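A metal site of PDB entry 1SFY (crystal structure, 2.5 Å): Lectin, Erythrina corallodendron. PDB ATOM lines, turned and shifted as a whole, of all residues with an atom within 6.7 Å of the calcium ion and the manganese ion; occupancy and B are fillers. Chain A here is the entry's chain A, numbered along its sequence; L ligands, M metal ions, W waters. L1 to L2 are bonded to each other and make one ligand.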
ATOM      1  N   ASP A  89     -32.052   4.461  18.478  1.00  0.00           N
ATOM      2  CA  ASP A  89     -30.659   4.127  18.160  1.00  0.00           C
ATOM      3  C   ASP A  89     -30.254   4.471  16.723  1.00  0.00           C
ATOM      4  O   ASP A  89     -29.069   4.713  16.453  1.00  0.00           O
ATOM      5  CB  ASP A  89     -30.431   2.632  18.407  1.00  0.00           C
ATOM      6  CG  ASP A  89     -30.025   2.322  19.824  1.00  0.00           C
ATOM      7  OD1 ASP A  89     -28.842   2.569  20.171  1.00  0.00           O
ATOM      8  OD2 ASP A  89     -30.889   1.863  20.606  1.00  0.00           O
ATOM      9  N   TYR A 106     -31.373  -2.189  19.656  1.00  0.00           N
ATOM     10  CA  TYR A 106     -30.499  -1.168  20.207  1.00  0.00           C
ATOM     11  C   TYR A 106     -29.350  -0.813  19.264  1.00  0.00           C
ATOM     12  O   TYR A 106     -29.541  -0.672  18.062  1.00  0.00           O
ATOM     13  CB  TYR A 106     -29.929  -1.632  21.551  1.00  0.00           C
ATOM     14  CG  TYR A 106     -30.960  -2.220  22.486  1.00  0.00           C
ATOM     15  CD1 TYR A 106     -32.169  -1.574  22.720  1.00  0.00           C
ATOM     16  CD2 TYR A 106     -30.708  -3.411  23.165  1.00  0.00           C
ATOM     17  CE1 TYR A 106     -33.112  -2.095  23.599  1.00  0.00           C
ATOM     18  CE2 TYR A 106     -31.641  -3.953  24.046  1.00  0.00           C
ATOM     19  CZ  TYR A 106     -32.837  -3.288  24.259  1.00  0.00           C
ATOM     20  OH  TYR A 106     -33.748  -3.818  25.139  1.00  0.00           O
ATOM     21  N   GLY A 107     -28.156  -0.681  19.823  1.00  0.00           N
ATOM     22  CA  GLY A 107     -26.992  -0.332  19.023  1.00  0.00           C
ATOM     23  C   GLY A 107     -26.702  -1.268  17.855  1.00  0.00           C
ATOM     24  O   GLY A 107     -25.965  -0.912  16.954  1.00  0.00           O
ATOM     25  N   TYR A 108     -27.285  -2.459  17.881  1.00  0.00           N
ATOM     26  CA  TYR A 108     -27.056  -3.420  16.802  1.00  0.00           C
ATOM     27  C   TYR A 108     -27.994  -3.175  15.630  1.00  0.00           C
ATOM     28  O   TYR A 108     -27.934  -3.878  14.605  1.00  0.00           O
ATOM     29  CB  TYR A 108     -27.188  -4.844  17.338  1.00  0.00           C
ATOM     30  CG  TYR A 108     -26.157  -5.120  18.416  1.00  0.00           C
ATOM     31  CD1 TYR A 108     -24.799  -5.122  18.120  1.00  0.00           C
ATOM     32  CD2 TYR A 108     -26.548  -5.289  19.748  1.00  0.00           C
ATOM     33  CE1 TYR A 108     -23.841  -5.267  19.119  1.00  0.00           C
ATOM     34  CE2 TYR A 108     -25.595  -5.441  20.751  1.00  0.00           C
ATOM     35  CZ  TYR A 108     -24.246  -5.435  20.434  1.00  0.00           C
ATOM     36  OH  TYR A 108     -23.304  -5.567  21.434  1.00  0.00           O
ATOM     37  N   LEU A 109     -28.849  -2.171  15.789  1.00  0.00           N
ATOM     38  CA  LEU A 109     -29.793  -1.752  14.755  1.00  0.00           C
ATOM     39  C   LEU A 109     -30.658  -2.845  14.144  1.00  0.00           C
ATOM     40  O   LEU A 109     -31.207  -2.668  13.062  1.00  0.00           O
ATOM     41  CB  LEU A 109     -29.032  -1.019  13.658  1.00  0.00           C
ATOM     42  CG  LEU A 109     -28.169   0.134  14.183  1.00  0.00           C
ATOM     43  CD1 LEU A 109     -27.510   0.864  13.027  1.00  0.00           C
ATOM     44  CD2 LEU A 109     -29.036   1.098  14.989  1.00  0.00           C
ATOM     45  N   GLU A 127     -25.475   2.793   7.821  1.00  0.00           N
ATOM     46  CA  GLU A 127     -26.185   3.270   8.998  1.00  0.00           C
ATOM     47  C   GLU A 127     -26.251   4.774   9.212  1.00  0.00           C
ATOM     48  O   GLU A 127     -25.380   5.529   8.782  1.00  0.00           O
ATOM     49  CB  GLU A 127     -25.593   2.643  10.261  1.00  0.00           C
ATOM     50  CG  GLU A 127     -24.127   2.991  10.440  1.00  0.00           C
ATOM     51  CD  GLU A 127     -23.604   2.654  11.819  1.00  0.00           C
ATOM     52  OE1 GLU A 127     -23.741   1.492  12.252  1.00  0.00           O
ATOM     53  OE2 GLU A 127     -23.040   3.556  12.454  1.00  0.00           O
ATOM     54  N   ASP A 129     -26.616   6.376  12.477  1.00  0.00           N
ATOM     55  CA  ASP A 129     -26.499   6.155  13.914  1.00  0.00           C
ATOM     56  C   ASP A 129     -26.722   7.380  14.773  1.00  0.00           C
ATOM     57  O   ASP A 129     -26.045   8.394  14.597  1.00  0.00           O
ATOM     58  CB  ASP A 129     -25.105   5.615  14.190  1.00  0.00           C
ATOM     59  CG  ASP A 129     -25.038   4.843  15.461  1.00  0.00           C
ATOM     60  OD1 ASP A 129     -25.796   5.163  16.393  1.00  0.00           O
ATOM     61  OD2 ASP A 129     -24.205   3.915  15.534  1.00  0.00           O
ATOM     62  N   THR A 130     -27.651   7.289  15.712  1.00  0.00           N
ATOM     63  CA  THR A 130     -27.959   8.428  16.575  1.00  0.00           C
ATOM     64  C   THR A 130     -27.488   8.314  18.028  1.00  0.00           C
ATOM     65  O   THR A 130     -27.627   9.260  18.806  1.00  0.00           O
ATOM     66  CB  THR A 130     -29.474   8.713  16.575  1.00  0.00           C
ATOM     67  OG1 THR A 130     -30.185   7.540  16.994  1.00  0.00           O
ATOM     68  CG2 THR A 130     -29.932   9.113  15.195  1.00  0.00           C
ATOM     69  N   PHE A 131     -26.927   7.169  18.389  1.00  0.00           N
ATOM     70  CA  PHE A 131     -26.423   6.971  19.743  1.00  0.00           C
ATOM     71  C   PHE A 131     -24.985   6.505  19.697  1.00  0.00           C
ATOM     72  O   PHE A 131     -24.625   5.655  18.890  1.00  0.00           O
ATOM     73  CB  PHE A 131     -27.266   5.946  20.494  1.00  0.00           C
ATOM     74  CG  PHE A 131     -26.841   5.767  21.918  1.00  0.00           C
ATOM     75  CD1 PHE A 131     -27.275   6.655  22.900  1.00  0.00           C
ATOM     76  CD2 PHE A 131     -25.986   4.738  22.283  1.00  0.00           C
ATOM     77  CE1 PHE A 131     -26.853   6.519  24.233  1.00  0.00           C
ATOM     78  CE2 PHE A 131     -25.547   4.593  23.601  1.00  0.00           C
ATOM     79  CZ  PHE A 131     -25.992   5.485  24.575  1.00  0.00           C
ATOM     80  N   SER A 132     -24.140   7.043  20.581  1.00  0.00           N
ATOM     81  CA  SER A 132     -22.734   6.639  20.595  1.00  0.00           C
ATOM     82  C   SER A 132     -22.457   5.466  21.539  1.00  0.00           C
ATOM     83  O   SER A 132     -22.450   5.636  22.751  1.00  0.00           O
ATOM     84  CB  SER A 132     -21.853   7.824  20.968  1.00  0.00           C
ATOM     85  OG  SER A 132     -20.483   7.504  20.779  1.00  0.00           O
ATOM     86  N   ASN A 133     -22.232   4.291  20.967  1.00  0.00           N
ATOM     87  CA  ASN A 133     -21.941   3.084  21.737  1.00  0.00           C
ATOM     88  C   ASN A 133     -20.428   2.963  21.956  1.00  0.00           C
ATOM     89  O   ASN A 133     -19.658   3.755  21.420  1.00  0.00           O
ATOM     90  CB  ASN A 133     -22.468   1.849  21.013  1.00  0.00           C
ATOM     91  CG  ASN A 133     -23.964   1.664  21.154  1.00  0.00           C
ATOM     92  OD1 ASN A 133     -24.743   2.496  20.720  1.00  0.00           O
ATOM     93  ND2 ASN A 133     -24.373   0.582  21.794  1.00  0.00           N
ATOM     94  N   TRP A 135     -18.371   1.083  20.705  1.00  0.00           N
ATOM     95  CA  TRP A 135     -17.703   0.869  19.428  1.00  0.00           C
ATOM     96  C   TRP A 135     -17.849   2.032  18.446  1.00  0.00           C
ATOM     97  O   TRP A 135     -17.292   1.985  17.351  1.00  0.00           O
ATOM     98  CB  TRP A 135     -18.219  -0.416  18.795  1.00  0.00           C
ATOM     99  CG  TRP A 135     -19.695  -0.383  18.522  1.00  0.00           C
ATOM    100  CD1 TRP A 135     -20.341   0.306  17.541  1.00  0.00           C
ATOM    101  CD2 TRP A 135     -20.723  -1.020  19.291  1.00  0.00           C
ATOM    102  NE1 TRP A 135     -21.700   0.134  17.645  1.00  0.00           N
ATOM    103  CE2 TRP A 135     -21.963  -0.670  18.712  1.00  0.00           C
ATOM    104  CE3 TRP A 135     -20.719  -1.860  20.419  1.00  0.00           C
ATOM    105  CZ2 TRP A 135     -23.180  -1.130  19.220  1.00  0.00           C
ATOM    106  CZ3 TRP A 135     -21.931  -2.313  20.924  1.00  0.00           C
ATOM    107  CH2 TRP A 135     -23.142  -1.941  20.325  1.00  0.00           C
ATOM    108  N   ASP A 136     -18.581   3.072  18.814  1.00  0.00           N
ATOM    109  CA  ASP A 136     -18.784   4.217  17.916  1.00  0.00           C
ATOM    110  C   ASP A 136     -17.856   5.382  18.176  1.00  0.00           C
ATOM    111  O   ASP A 136     -17.271   5.501  19.240  1.00  0.00           O
ATOM    112  CB  ASP A 136     -20.205   4.785  18.036  1.00  0.00           C
ATOM    113  CG  ASP A 136     -21.368   4.104  17.415  1.00  0.00           C
ATOM    114  OD1 ASP A 136     -21.309   3.791  16.210  1.00  0.00           O
ATOM    115  OD2 ASP A 136     -22.363   3.894  18.126  1.00  0.00           O
ATOM    116  N   PRO A 137     -17.715   6.264  17.179  1.00  0.00           N
ATOM    117  CA  PRO A 137     -16.856   7.421  17.368  1.00  0.00           C
ATOM    118  C   PRO A 137     -17.691   8.324  18.292  1.00  0.00           C
ATOM    119  O   PRO A 137     -18.884   8.089  18.473  1.00  0.00           O
ATOM    120  CB  PRO A 137     -16.722   7.986  15.958  1.00  0.00           C
ATOM    121  CG  PRO A 137     -17.983   7.572  15.290  1.00  0.00           C
ATOM    122  CD  PRO A 137     -18.133   6.152  15.765  1.00  0.00           C
ATOM    123  N   VAL A 140     -22.281  11.965  17.104  1.00  0.00           N
ATOM    124  CA  VAL A 140     -23.553  11.403  16.679  1.00  0.00           C
ATOM    125  C   VAL A 140     -24.460  12.592  16.397  1.00  0.00           C
ATOM    126  O   VAL A 140     -24.363  13.620  17.055  1.00  0.00           O
ATOM    127  CB  VAL A 140     -24.212  10.498  17.756  1.00  0.00           C
ATOM    128  CG1 VAL A 140     -23.440   9.202  17.902  1.00  0.00           C
ATOM    129  CG2 VAL A 140     -24.297  11.245  19.092  1.00  0.00           C
ATOM    130  N   HIS A 142     -24.166   9.967  13.012  1.00  0.00           N
ATOM    131  CA  HIS A 142     -23.136   9.782  11.996  1.00  0.00           C
ATOM    132  C   HIS A 142     -23.579   8.741  10.987  1.00  0.00           C
ATOM    133  O   HIS A 142     -24.379   7.857  11.294  1.00  0.00           O
ATOM    134  CB  HIS A 142     -21.801   9.365  12.626  1.00  0.00           C
ATOM    135  CG  HIS A 142     -21.853   8.065  13.372  1.00  0.00           C
ATOM    136  ND1 HIS A 142     -21.907   7.994  14.751  1.00  0.00           N
ATOM    137  CD2 HIS A 142     -21.818   6.780  12.933  1.00  0.00           C
ATOM    138  CE1 HIS A 142     -21.914   6.729  15.131  1.00  0.00           C
ATOM    139  NE2 HIS A 142     -21.855   5.973  14.044  1.00  0.00           N
ATOM    140  N   ILE A 143     -23.079   8.882   9.766  1.00  0.00           N
ATOM    141  CA  ILE A 143     -23.359   7.920   8.700  1.00  0.00           C
ATOM    142  C   ILE A 143     -22.215   6.919   8.805  1.00  0.00           C
ATOM    143  O   ILE A 143     -21.072   7.321   9.063  1.00  0.00           O
ATOM    144  CB  ILE A 143     -23.296   8.555   7.296  1.00  0.00           C
ATOM    145  CG1 ILE A 143     -24.231   9.754   7.224  1.00  0.00           C
ATOM    146  CG2 ILE A 143     -23.664   7.532   6.251  1.00  0.00           C
ATOM    147  CD1 ILE A 143     -24.081  10.537   5.940  1.00  0.00           C
ATOM    148  N   GLY A 144     -22.503   5.645   8.627  1.00  0.00           N
ATOM    149  CA  GLY A 144     -21.447   4.665   8.727  1.00  0.00           C
ATOM    150  C   GLY A 144     -21.635   3.533   7.746  1.00  0.00           C
ATOM    151  O   GLY A 144     -22.762   3.124   7.451  1.00  0.00           O
ATOM    152  N   ASP A 146     -21.078  -0.237   7.232  1.00  0.00           N
ATOM    153  CA  ASP A 146     -20.876  -1.457   8.008  1.00  0.00           C
ATOM    154  C   ASP A 146     -20.677  -2.697   7.164  1.00  0.00           C
ATOM    155  O   ASP A 146     -21.542  -3.073   6.383  1.00  0.00           O
ATOM    156  CB  ASP A 146     -22.052  -1.674   8.962  1.00  0.00           C
ATOM    157  CG  ASP A 146     -22.308  -0.480   9.866  1.00  0.00           C
ATOM    158  OD1 ASP A 146     -21.420   0.392   9.988  1.00  0.00           O
ATOM    159  OD2 ASP A 146     -23.395  -0.408  10.469  1.00  0.00           O
ATOM    160  N   ILE A 150     -20.918  -4.112  13.353  1.00  0.00           N
ATOM    161  CA  ILE A 150     -21.580  -2.880  13.734  1.00  0.00           C
ATOM    162  C   ILE A 150     -20.528  -1.783  13.876  1.00  0.00           C
ATOM    163  O   ILE A 150     -20.854  -0.597  13.935  1.00  0.00           O
ATOM    164  CB  ILE A 150     -22.337  -3.034  15.073  1.00  0.00           C
ATOM    165  CG1 ILE A 150     -23.190  -1.794  15.348  1.00  0.00           C
ATOM    166  CG2 ILE A 150     -21.353  -3.265  16.212  1.00  0.00           C
ATOM    167  CD1 ILE A 150     -24.281  -1.537  14.323  1.00  0.00           C
ATOM    168  N   ARG A 151     -19.262  -2.175  13.942  1.00  0.00           N
ATOM    169  CA  ARG A 151     -18.179  -1.204  14.033  1.00  0.00           C
ATOM    170  C   ARG A 151     -17.806  -0.793  12.620  1.00  0.00           C
ATOM    171  O   ARG A 151     -17.070  -1.491  11.929  1.00  0.00           O
ATOM    172  CB  ARG A 151     -16.915  -1.627  14.749  1.00  0.00           C
ATOM    173  CG  ARG A 151     -15.864  -0.600  15.026  1.00  0.00           C
ATOM    174  CD  ARG A 151     -14.954  -0.903  16.251  1.00  0.00           C
ATOM    175  NE  ARG A 151     -14.803  -2.116  17.090  1.00  0.00           N
ATOM    176  CZ  ARG A 151     -15.734  -2.984  17.489  1.00  0.00           C
ATOM    177  NH1 ARG A 151     -16.165  -3.972  16.717  1.00  0.00           N
ATOM    178  NH2 ARG A 151     -16.244  -2.820  18.696  1.00  0.00           N
ATOM    179  N   SER A 152     -18.328   0.349  12.188  1.00  0.00           N
ATOM    180  CA  SER A 152     -18.102   0.871  10.844  1.00  0.00           C
ATOM    181  C   SER A 152     -16.641   0.935  10.419  1.00  0.00           C
ATOM    182  O   SER A 152     -15.773   1.197  11.246  1.00  0.00           O
ATOM    183  CB  SER A 152     -18.703   2.275  10.719  1.00  0.00           C
ATOM    184  OG  SER A 152     -20.044   2.292  11.150  1.00  0.00           O
ATOM    185  N   THR A 155     -16.726   6.335   8.859  1.00  0.00           N
ATOM    186  CA  THR A 155     -17.743   7.105   9.551  1.00  0.00           C
ATOM    187  C   THR A 155     -17.769   8.561   9.101  1.00  0.00           C
ATOM    188  O   THR A 155     -16.756   9.122   8.687  1.00  0.00           O
ATOM    189  CB  THR A 155     -17.488   7.019  11.080  1.00  0.00           C
ATOM    190  OG1 THR A 155     -18.362   6.034  11.651  1.00  0.00           O
ATOM    191  CG2 THR A 155     -17.666   8.360  11.750  1.00  0.00           C
HETATM  192  C1  LIG L   1     -28.789   0.927  30.467  1.00  0.00           C
HETATM  193  C2  LIG L   1     -29.118   0.678  29.005  1.00  0.00           C
HETATM  194  C3  LIG L   1     -27.743   0.489  28.245  1.00  0.00           C
HETATM  195  C4  LIG L   1     -26.904  -0.691  28.843  1.00  0.00           C
HETATM  196  C5  LIG L   1     -25.434  -0.884  28.327  1.00  0.00           C
HETATM  197  C6  LIG L   1     -28.012  -0.288  31.022  1.00  0.00           C
HETATM  198  O1  LIG L   1     -27.668  -0.114  32.379  1.00  0.00           O
HETATM  199  O2  LIG L   1     -30.010   1.121  31.174  1.00  0.00           O
HETATM  200  O3  LIG L   1     -29.858   1.792  28.488  1.00  0.00           O
HETATM  201  O4  LIG L   1     -27.971   0.196  26.835  1.00  0.00           O
HETATM  202  O5  LIG L   1     -26.790  -0.506  30.277  1.00  0.00           O
HETATM  203  O6  LIG L   1     -24.609   0.296  28.601  1.00  0.00           O
HETATM  204  C1  LG2 L   2     -27.800   1.222  25.859  1.00  0.00           C
HETATM  205  C2  LG2 L   2     -27.747   0.572  24.460  1.00  0.00           C
HETATM  206  C3  LG2 L   2     -27.568   1.685  23.386  1.00  0.00           C
HETATM  207  C4  LG2 L   2     -28.784   2.669  23.528  1.00  0.00           C
HETATM  208  C5  LG2 L   2     -28.820   3.270  24.958  1.00  0.00           C
HETATM  209  C6  LG2 L   2     -30.015   4.219  25.181  1.00  0.00           C
HETATM  210  O1  LG2 L   2     -26.671  -0.348  24.343  1.00  0.00           O
HETATM  211  O2  LG2 L   2     -27.516   1.100  22.069  1.00  0.00           O
HETATM  212  O3  LG2 L   2     -30.027   1.978  23.245  1.00  0.00           O
HETATM  213  O4  LG2 L   2     -28.891   2.178  25.926  1.00  0.00           O
HETATM  214  O5  LG2 L   2     -29.956   4.718  26.492  1.00  0.00           O
HETATM  215 CA    CA M   1     -24.819   3.223  18.029  1.00  0.00          CA
HETATM  216 MN    MN M   2     -22.132   3.745  14.500  1.00  0.00          MN
HETATM  217  O   HOH W   1     -24.898   1.139  16.856  1.00  0.00           O
HETATM  218  O   HOH W   2     -22.591   1.466  14.786  1.00  0.00           O
HETATM  219  O   HOH W   3     -27.550   3.369  18.043  1.00  0.00           O
HETATM  220  O   HOH W   4     -20.217   3.527  13.556  1.00  0.00           O
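The calcium ion is bound by water W1, 2.4 Å away. OD2 of Asp 136 binds the calcium ion (2.5 Å). The calcium ion is bound by O of Phe 131 (2.6 Å). The calcium ion is bound by OD2 of Asp 129. The calcium ion is bound by OD1 of Asp 129 (2.7 Å). Water W3 is bound to the calcium ion (2.7 Å). The calcium ion is bound by OD1 of Asn 133 (2.8 Å). The calcium ion has seven donor atoms within binding distance.
OD2 of Asp 146 lies close to OE1 of Glu 127 (2.6 Å). N of Glu 127 sits at hydrogen-bond distance from O of Gly 144, 2.8 Å away.
The nearest printed residue that does not touch the calcium ion is Gly 107 (4.3 Å).
Four residues have an atom within 4 Å of the manganese ion: Glu 127, Asp 129, Asp 136 and His 142.
Water W2 lies within hydrogen-bond range of the side-chain carboxylate (OE1) of Glu 127 (2.8 Å), the backbone carbonyl oxygen (O) of Ile 150 (2.8 Å) and the indole nitrogen (NE1) of Trp 135 (3.3 Å).
The manganese ion is bound by the side-chain carboxylate of Asp 136 (1.9 Å), water W4 (2.1 Å), the side-chain carboxylate of Glu 127 (2.2 Å), a ring nitrogen (NE2) of His 142 (2.3 Å), the side-chain carboxylate of Asp 129 (2.3 Å) and water W2 (2.3 Å). The manganese ion has six donor atoms within binding distance.
The backbone NH (N) of Gly 107 sits at hydrogen-bond distance from an oxygen (O2) of LG2 L2 (2.9 Å). The side-chain amide nitrogen (ND2) of Asn 133 lies within hydrogen-bond range of an oxygen (O2) of LG2 L2 (3.2 Å). The side-chain carboxylate (OD1) of Asp 89 is in hydrogen-bond range of an oxygen (O2) of LG2 L2, at 2.7 Å.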
